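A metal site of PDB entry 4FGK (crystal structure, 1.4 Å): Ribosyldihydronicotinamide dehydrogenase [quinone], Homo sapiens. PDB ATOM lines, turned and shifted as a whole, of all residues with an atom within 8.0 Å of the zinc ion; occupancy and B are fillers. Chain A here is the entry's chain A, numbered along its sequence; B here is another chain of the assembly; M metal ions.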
ATOM      1  N   TYR A 135      10.172  -7.237   4.825  1.00  0.00           N
ATOM      2  CA  TYR A 135      10.084  -6.104   3.892  1.00  0.00           C
ATOM      3  C   TYR A 135      10.920  -6.407   2.627  1.00  0.00           C
ATOM      4  O   TYR A 135      10.672  -7.432   1.991  1.00  0.00           O
ATOM      5  CB  TYR A 135      10.364  -4.761   4.569  1.00  0.00           C
ATOM      6  CG  TYR A 135       9.184  -4.358   5.439  1.00  0.00           C
ATOM      7  CD1 TYR A 135       7.911  -4.257   4.893  1.00  0.00           C
ATOM      8  CD2 TYR A 135       9.330  -4.114   6.800  1.00  0.00           C
ATOM      9  CE1 TYR A 135       6.817  -3.925   5.679  1.00  0.00           C
ATOM     10  CE2 TYR A 135       8.249  -3.767   7.587  1.00  0.00           C
ATOM     11  CZ  TYR A 135       6.992  -3.679   7.018  1.00  0.00           C
ATOM     12  OH  TYR A 135       5.895  -3.357   7.795  1.00  0.00           O
ATOM     13  N   ASP A 136      11.894  -5.576   2.260  1.00  0.00           N
ATOM     14  CA  ASP A 136      12.607  -5.823   0.992  1.00  0.00           C
ATOM     15  C   ASP A 136      13.284  -7.190   0.917  1.00  0.00           C
ATOM     16  O   ASP A 136      13.488  -7.734  -0.171  1.00  0.00           O
ATOM     17  CB  ASP A 136      13.626  -4.716   0.703  1.00  0.00           C
ATOM     18  CG  ASP A 136      12.980  -3.378   0.372  1.00  0.00           C
ATOM     19  OD1 ASP A 136      11.744  -3.358   0.196  1.00  0.00           O
ATOM     20  OD2 ASP A 136      13.687  -2.355   0.288  1.00  0.00           O
ATOM     21  N   TRP A 172      -2.847  -0.062   3.344  1.00  0.00           N
ATOM     22  CA  TRP A 172      -1.636  -0.191   4.158  1.00  0.00           C
ATOM     23  C   TRP A 172      -1.461  -1.560   4.822  1.00  0.00           C
ATOM     24  O   TRP A 172      -0.401  -2.167   4.679  1.00  0.00           O
ATOM     25  CB  TRP A 172      -1.597   0.942   5.174  1.00  0.00           C
ATOM     26  CG  TRP A 172      -0.459   0.977   6.117  1.00  0.00           C
ATOM     27  CD1 TRP A 172      -0.516   0.773   7.476  1.00  0.00           C
ATOM     28  CD2 TRP A 172       0.887   1.328   5.825  1.00  0.00           C
ATOM     29  NE1 TRP A 172       0.718   0.959   8.034  1.00  0.00           N
ATOM     30  CE2 TRP A 172       1.604   1.304   7.050  1.00  0.00           C
ATOM     31  CE3 TRP A 172       1.580   1.653   4.658  1.00  0.00           C
ATOM     32  CZ2 TRP A 172       2.969   1.589   7.129  1.00  0.00           C
ATOM     33  CZ3 TRP A 172       2.932   1.937   4.734  1.00  0.00           C
ATOM     34  CH2 TRP A 172       3.605   1.898   5.958  1.00  0.00           C
ATOM     35  N   LEU A 174      -2.659  -4.401   4.121  1.00  0.00           N
ATOM     36  CA  LEU A 174      -2.602  -5.461   3.132  1.00  0.00           C
ATOM     37  C   LEU A 174      -1.326  -5.376   2.283  1.00  0.00           C
ATOM     38  O   LEU A 174      -0.542  -6.331   2.218  1.00  0.00           O
ATOM     39  CB  LEU A 174      -3.833  -5.389   2.238  1.00  0.00           C
ATOM     40  CG  LEU A 174      -5.175  -5.541   2.939  1.00  0.00           C
ATOM     41  CD1 LEU A 174      -6.312  -5.307   1.961  1.00  0.00           C
ATOM     42  CD2 LEU A 174      -5.297  -6.912   3.554  1.00  0.00           C
ATOM     43  N   GLN A 175      -1.095  -4.220   1.652  1.00  0.00           N
ATOM     44  CA  GLN A 175       0.047  -4.055   0.779  1.00  0.00           C
ATOM     45  C   GLN A 175       1.349  -4.021   1.541  1.00  0.00           C
ATOM     46  O   GLN A 175       2.298  -4.703   1.162  1.00  0.00           O
ATOM     47  CB  GLN A 175      -0.077  -2.786  -0.081  1.00  0.00           C
ATOM     48  CG  GLN A 175      -1.212  -2.874  -1.064  1.00  0.00           C
ATOM     49  CD  GLN A 175      -1.205  -1.803  -2.134  1.00  0.00           C
ATOM     50  OE1 GLN A 175      -1.723  -2.016  -3.208  1.00  0.00           O
ATOM     51  NE2 GLN A 175      -0.653  -0.627  -1.810  1.00  0.00           N
ATOM     52  N   HIS A 176       1.379  -3.230   2.617  1.00  0.00           N
ATOM     53  CA  HIS A 176       2.626  -3.039   3.364  1.00  0.00           C
ATOM     54  C   HIS A 176       2.789  -4.039   4.508  1.00  0.00           C
ATOM     55  O   HIS A 176       3.779  -4.770   4.568  1.00  0.00           O
ATOM     56  CB  HIS A 176       2.726  -1.610   3.902  1.00  0.00           C
ATOM     57  CG  HIS A 176       4.017  -1.308   4.572  1.00  0.00           C
ATOM     58  ND1 HIS A 176       5.178  -1.076   3.875  1.00  0.00           N
ATOM     59  CD2 HIS A 176       4.340  -1.190   5.885  1.00  0.00           C
ATOM     60  CE1 HIS A 176       6.173  -0.857   4.722  1.00  0.00           C
ATOM     61  NE2 HIS A 176       5.682  -0.896   5.943  1.00  0.00           N
ATOM     62  N   GLY A 177       1.823  -4.081   5.422  1.00  0.00           N
ATOM     63  CA  GLY A 177       1.939  -4.920   6.596  1.00  0.00           C
ATOM     64  C   GLY A 177       1.923  -6.411   6.298  1.00  0.00           C
ATOM     65  O   GLY A 177       2.412  -7.199   7.112  1.00  0.00           O
ATOM     66  N   THR A 178       1.385  -6.803   5.153  1.00  0.00           N
ATOM     67  CA  THR A 178       1.321  -8.220   4.776  1.00  0.00           C
ATOM     68  C   THR A 178       2.232  -8.526   3.582  1.00  0.00           C
ATOM     69  O   THR A 178       3.237  -9.221   3.725  1.00  0.00           O
ATOM     70  CB  THR A 178      -0.137  -8.652   4.495  1.00  0.00           C
ATOM     71  OG1 THR A 178      -0.966  -8.307   5.610  1.00  0.00           O
ATOM     72  CG2 THR A 178      -0.208 -10.149   4.233  1.00  0.00           C
ATOM     73  N   LEU A 179       1.892  -7.997   2.406  1.00  0.00           N
ATOM     74  CA  LEU A 179       2.616  -8.377   1.187  1.00  0.00           C
ATOM     75  C   LEU A 179       4.079  -7.905   1.167  1.00  0.00           C
ATOM     76  O   LEU A 179       4.983  -8.719   0.989  1.00  0.00           O
ATOM     77  CB  LEU A 179       1.883  -7.857  -0.036  1.00  0.00           C
ATOM     78  CG  LEU A 179       0.474  -8.432  -0.222  1.00  0.00           C
ATOM     79  CD1 LEU A 179      -0.216  -7.779  -1.409  1.00  0.00           C
ATOM     80  CD2 LEU A 179       0.455  -9.945  -0.319  1.00  0.00           C
ATOM     81  N   HIS A 180       4.308  -6.608   1.348  1.00  0.00           N
ATOM     82  CA  HIS A 180       5.671  -6.094   1.413  1.00  0.00           C
ATOM     83  C   HIS A 180       6.422  -6.796   2.546  1.00  0.00           C
ATOM     84  O   HIS A 180       7.602  -7.135   2.390  1.00  0.00           O
ATOM     85  CB  HIS A 180       5.655  -4.581   1.596  1.00  0.00           C
ATOM     86  CG  HIS A 180       7.001  -3.921   1.488  1.00  0.00           C
ATOM     87  ND1 HIS A 180       7.164  -2.561   1.576  1.00  0.00           N
ATOM     88  CD2 HIS A 180       8.235  -4.436   1.264  1.00  0.00           C
ATOM     89  CE1 HIS A 180       8.447  -2.257   1.448  1.00  0.00           C
ATOM     90  NE2 HIS A 180       9.113  -3.382   1.264  1.00  0.00           N
ATOM     91  N   PHE A 181       5.768  -6.981   3.692  1.00  0.00           N
ATOM     92  CA  PHE A 181       6.424  -7.614   4.818  1.00  0.00           C
ATOM     93  C   PHE A 181       7.032  -8.955   4.418  1.00  0.00           C
ATOM     94  O   PHE A 181       8.119  -9.313   4.854  1.00  0.00           O
ATOM     95  CB  PHE A 181       5.467  -7.787   5.996  1.00  0.00           C
ATOM     96  CG  PHE A 181       6.131  -8.233   7.253  1.00  0.00           C
ATOM     97  CD1 PHE A 181       6.809  -7.330   8.049  1.00  0.00           C
ATOM     98  CD2 PHE A 181       6.081  -9.562   7.654  1.00  0.00           C
ATOM     99  CE1 PHE A 181       7.414  -7.733   9.220  1.00  0.00           C
ATOM    100  CE2 PHE A 181       6.696  -9.973   8.820  1.00  0.00           C
ATOM    101  CZ  PHE A 181       7.361  -9.058   9.608  1.00  0.00           C
ATOM    102  N   PHE A 184       7.187  -9.539  -1.116  1.00  0.00           N
ATOM    103  CA  PHE A 184       6.598  -9.276  -2.411  1.00  0.00           C
ATOM    104  C   PHE A 184       6.946  -7.861  -2.859  1.00  0.00           C
ATOM    105  O   PHE A 184       6.997  -6.926  -2.052  1.00  0.00           O
ATOM    106  CB  PHE A 184       5.076  -9.376  -2.384  1.00  0.00           C
ATOM    107  CG  PHE A 184       4.505 -10.761  -2.293  1.00  0.00           C
ATOM    108  CD1 PHE A 184       4.401 -11.564  -3.413  1.00  0.00           C
ATOM    109  CD2 PHE A 184       3.978 -11.234  -1.086  1.00  0.00           C
ATOM    110  CE1 PHE A 184       3.826 -12.823  -3.343  1.00  0.00           C
ATOM    111  CE2 PHE A 184       3.396 -12.501  -1.017  1.00  0.00           C
ATOM    112  CZ  PHE A 184       3.325 -13.292  -2.150  1.00  0.00           C
ATOM    113  N   VAL A 186       4.998  -5.076  -4.843  1.00  0.00           N
ATOM    114  CA  VAL A 186       3.581  -4.860  -4.957  1.00  0.00           C
ATOM    115  C   VAL A 186       3.255  -4.085  -6.199  1.00  0.00           C
ATOM    116  O   VAL A 186       3.683  -2.956  -6.375  1.00  0.00           O
ATOM    117  CB  VAL A 186       3.081  -4.105  -3.709  1.00  0.00           C
ATOM    118  CG1 VAL A 186       1.584  -3.820  -3.780  1.00  0.00           C
ATOM    119  CG2 VAL A 186       3.387  -4.916  -2.464  1.00  0.00           C
ATOM    120  N   ILE A 223       4.879  -0.502  -7.254  1.00  0.00           N
ATOM    121  CA  ILE A 223       4.809   0.759  -6.537  1.00  0.00           C
ATOM    122  C   ILE A 223       5.912   0.805  -5.489  1.00  0.00           C
ATOM    123  O   ILE A 223       6.421  -0.230  -5.075  1.00  0.00           O
ATOM    124  CB  ILE A 223       3.463   0.941  -5.780  1.00  0.00           C
ATOM    125  CG1 ILE A 223       3.312  -0.113  -4.666  1.00  0.00           C
ATOM    126  CG2 ILE A 223       2.294   0.908  -6.745  1.00  0.00           C
ATOM    127  CD1 ILE A 223       2.088   0.088  -3.784  1.00  0.00           C
ATOM    128  N   PRO A 224       6.288   2.023  -5.074  1.00  0.00           N
ATOM    129  CA  PRO A 224       7.117   2.103  -3.879  1.00  0.00           C
ATOM    130  C   PRO A 224       6.221   1.914  -2.654  1.00  0.00           C
ATOM    131  O   PRO A 224       5.432   2.805  -2.325  1.00  0.00           O
ATOM    132  CB  PRO A 224       7.694   3.521  -3.955  1.00  0.00           C
ATOM    133  CG  PRO A 224       6.642   4.318  -4.673  1.00  0.00           C
ATOM    134  CD  PRO A 224       5.916   3.345  -5.598  1.00  0.00           C
ATOM    135  N   CYS A 225       6.310   0.756  -2.019  1.00  0.00           N
ATOM    136  CA  CYS A 225       5.380   0.405  -0.940  1.00  0.00           C
ATOM    137  C   CYS A 225       5.828   1.054   0.361  1.00  0.00           C
ATOM    138  O   CYS A 225       6.391   0.411   1.251  1.00  0.00           O
ATOM    139  CB  CYS A 225       5.265  -1.105  -0.788  1.00  0.00           C
ATOM    140  SG  CYS A 225       3.916  -1.595   0.310  1.00  0.00           S
ATOM    141  N   THR A 226       5.582   2.350   0.420  1.00  0.00           N
ATOM    142  CA  THR A 226       6.058   3.186   1.510  1.00  0.00           C
ATOM    143  C   THR A 226       4.913   3.930   2.197  1.00  0.00           C
ATOM    144  O   THR A 226       3.819   4.074   1.638  1.00  0.00           O
ATOM    145  CB  THR A 226       7.041   4.259   0.976  1.00  0.00           C
ATOM    146  OG1 THR A 226       6.353   5.108   0.067  1.00  0.00           O
ATOM    147  CG2 THR A 226       8.236   3.605   0.294  1.00  0.00           C
ATOM    148  N   ALA A 227       5.180   4.438   3.383  1.00  0.00           N
ATOM    149  CA  ALA A 227       4.225   5.266   4.105  1.00  0.00           C
ATOM    150  C   ALA A 227       3.864   6.489   3.250  1.00  0.00           C
ATOM    151  O   ALA A 227       2.706   6.888   3.181  1.00  0.00           O
ATOM    152  CB  ALA A 227       4.782   5.695   5.455  1.00  0.00           C
ATOM    153  N   TRP A 229       3.760   6.790  -0.050  1.00  0.00           N
ATOM    154  CA  TRP A 229       2.850   6.414  -1.112  1.00  0.00           C
ATOM    155  C   TRP A 229       1.429   6.287  -0.564  1.00  0.00           C
ATOM    156  O   TRP A 229       0.476   6.739  -1.184  1.00  0.00           O
ATOM    157  CB  TRP A 229       3.294   5.098  -1.749  1.00  0.00           C
ATOM    158  CG  TRP A 229       2.485   4.695  -2.954  1.00  0.00           C
ATOM    159  CD1 TRP A 229       2.783   4.951  -4.263  1.00  0.00           C
ATOM    160  CD2 TRP A 229       1.261   3.947  -2.967  1.00  0.00           C
ATOM    161  NE1 TRP A 229       1.817   4.423  -5.089  1.00  0.00           N
ATOM    162  CE2 TRP A 229       0.878   3.791  -4.313  1.00  0.00           C
ATOM    163  CE3 TRP A 229       0.445   3.394  -1.972  1.00  0.00           C
ATOM    164  CZ2 TRP A 229      -0.279   3.126  -4.693  1.00  0.00           C
ATOM    165  CZ3 TRP A 229      -0.712   2.716  -2.348  1.00  0.00           C
ATOM    166  CH2 TRP A 229      -1.059   2.581  -3.698  1.00  0.00           C
ATOM    167  N   HIS A 230       1.306   5.686   0.609  1.00  0.00           N
ATOM    168  CA  HIS A 230      -0.016   5.418   1.171  1.00  0.00           C
ATOM    169  C   HIS A 230      -0.677   6.660   1.785  1.00  0.00           C
ATOM    170  O   HIS A 230      -1.884   6.839   1.656  1.00  0.00           O
ATOM    171  CB  HIS A 230       0.066   4.296   2.209  1.00  0.00           C
ATOM    172  CG  HIS A 230       0.275   2.931   1.621  1.00  0.00           C
ATOM    173  ND1 HIS A 230       1.517   2.441   1.296  1.00  0.00           N
ATOM    174  CD2 HIS A 230      -0.605   1.934   1.356  1.00  0.00           C
ATOM    175  CE1 HIS A 230       1.393   1.217   0.817  1.00  0.00           C
ATOM    176  NE2 HIS A 230       0.120   0.885   0.836  1.00  0.00           N
ATOM    177  N   VAL B 163       9.923   1.475   9.564  1.00  0.00           N
ATOM    178  CA  VAL B 163       9.382   0.917   8.339  1.00  0.00           C
ATOM    179  C   VAL B 163       7.928   0.413   8.523  1.00  0.00           C
ATOM    180  O   VAL B 163       7.123   0.498   7.600  1.00  0.00           O
ATOM    181  CB  VAL B 163      10.285  -0.194   7.767  1.00  0.00           C
ATOM    182  CG1 VAL B 163       9.749  -0.684   6.439  1.00  0.00           C
ATOM    183  CG2 VAL B 163      11.692   0.336   7.604  1.00  0.00           C
HETATM  184 ZN    ZN M   1       5.512  -1.335   1.890  1.00  0.00          ZN
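Thr 226 touches the zinc ion (N to ZN, 3.97 Å). Of the 21 residues printed, 4 come within 4 Å of the zinc ion. The nearest printed residue that does not touch the zinc ion is Gln 175 (4.7 Å).
A ring nitrogen (ND1) of His 176 binds the zinc ion, at 2.0 Å. The backbone carbonyl oxygen (O) of Cys 225 binds the zinc ion (2.1 Å). ND1 of His 180 binds the zinc ion (2.1 Å). The zinc ion is bound by SG of Cys 225 (2.3 Å).
A ring nitrogen (NE2) of His 176 sits at hydrogen-bond distance from the side-chain hydroxyl (OH) of Tyr 135, 3.1 Å away. OG1 of Thr 226 is in hydrogen-bond range of O of Pro 224 (3.4 Å). The backbone carbonyl oxygen (O) of Val 163 of chain B lies within hydrogen-bond range of a ring nitrogen (NE2) of His 176 (2.6 Å). OD1 of Asp 136 sits at hydrogen-bond distance from NE2 of His 180 (2.8 Å). SG of Cys 225 sits close to O of Gln 175 (3.6 Å). O of Thr 226 is in hydrogen-bond range of ND1 of His 230 (2.8 Å). The backbone NH (N) of Phe 181 sits at hydrogen-bond distance from the backbone carbonyl oxygen (O) of His 176 (3.1 Å). OG1 of Thr 226 is in hydrogen-bond range of N of Trp 229 (3.1 Å).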
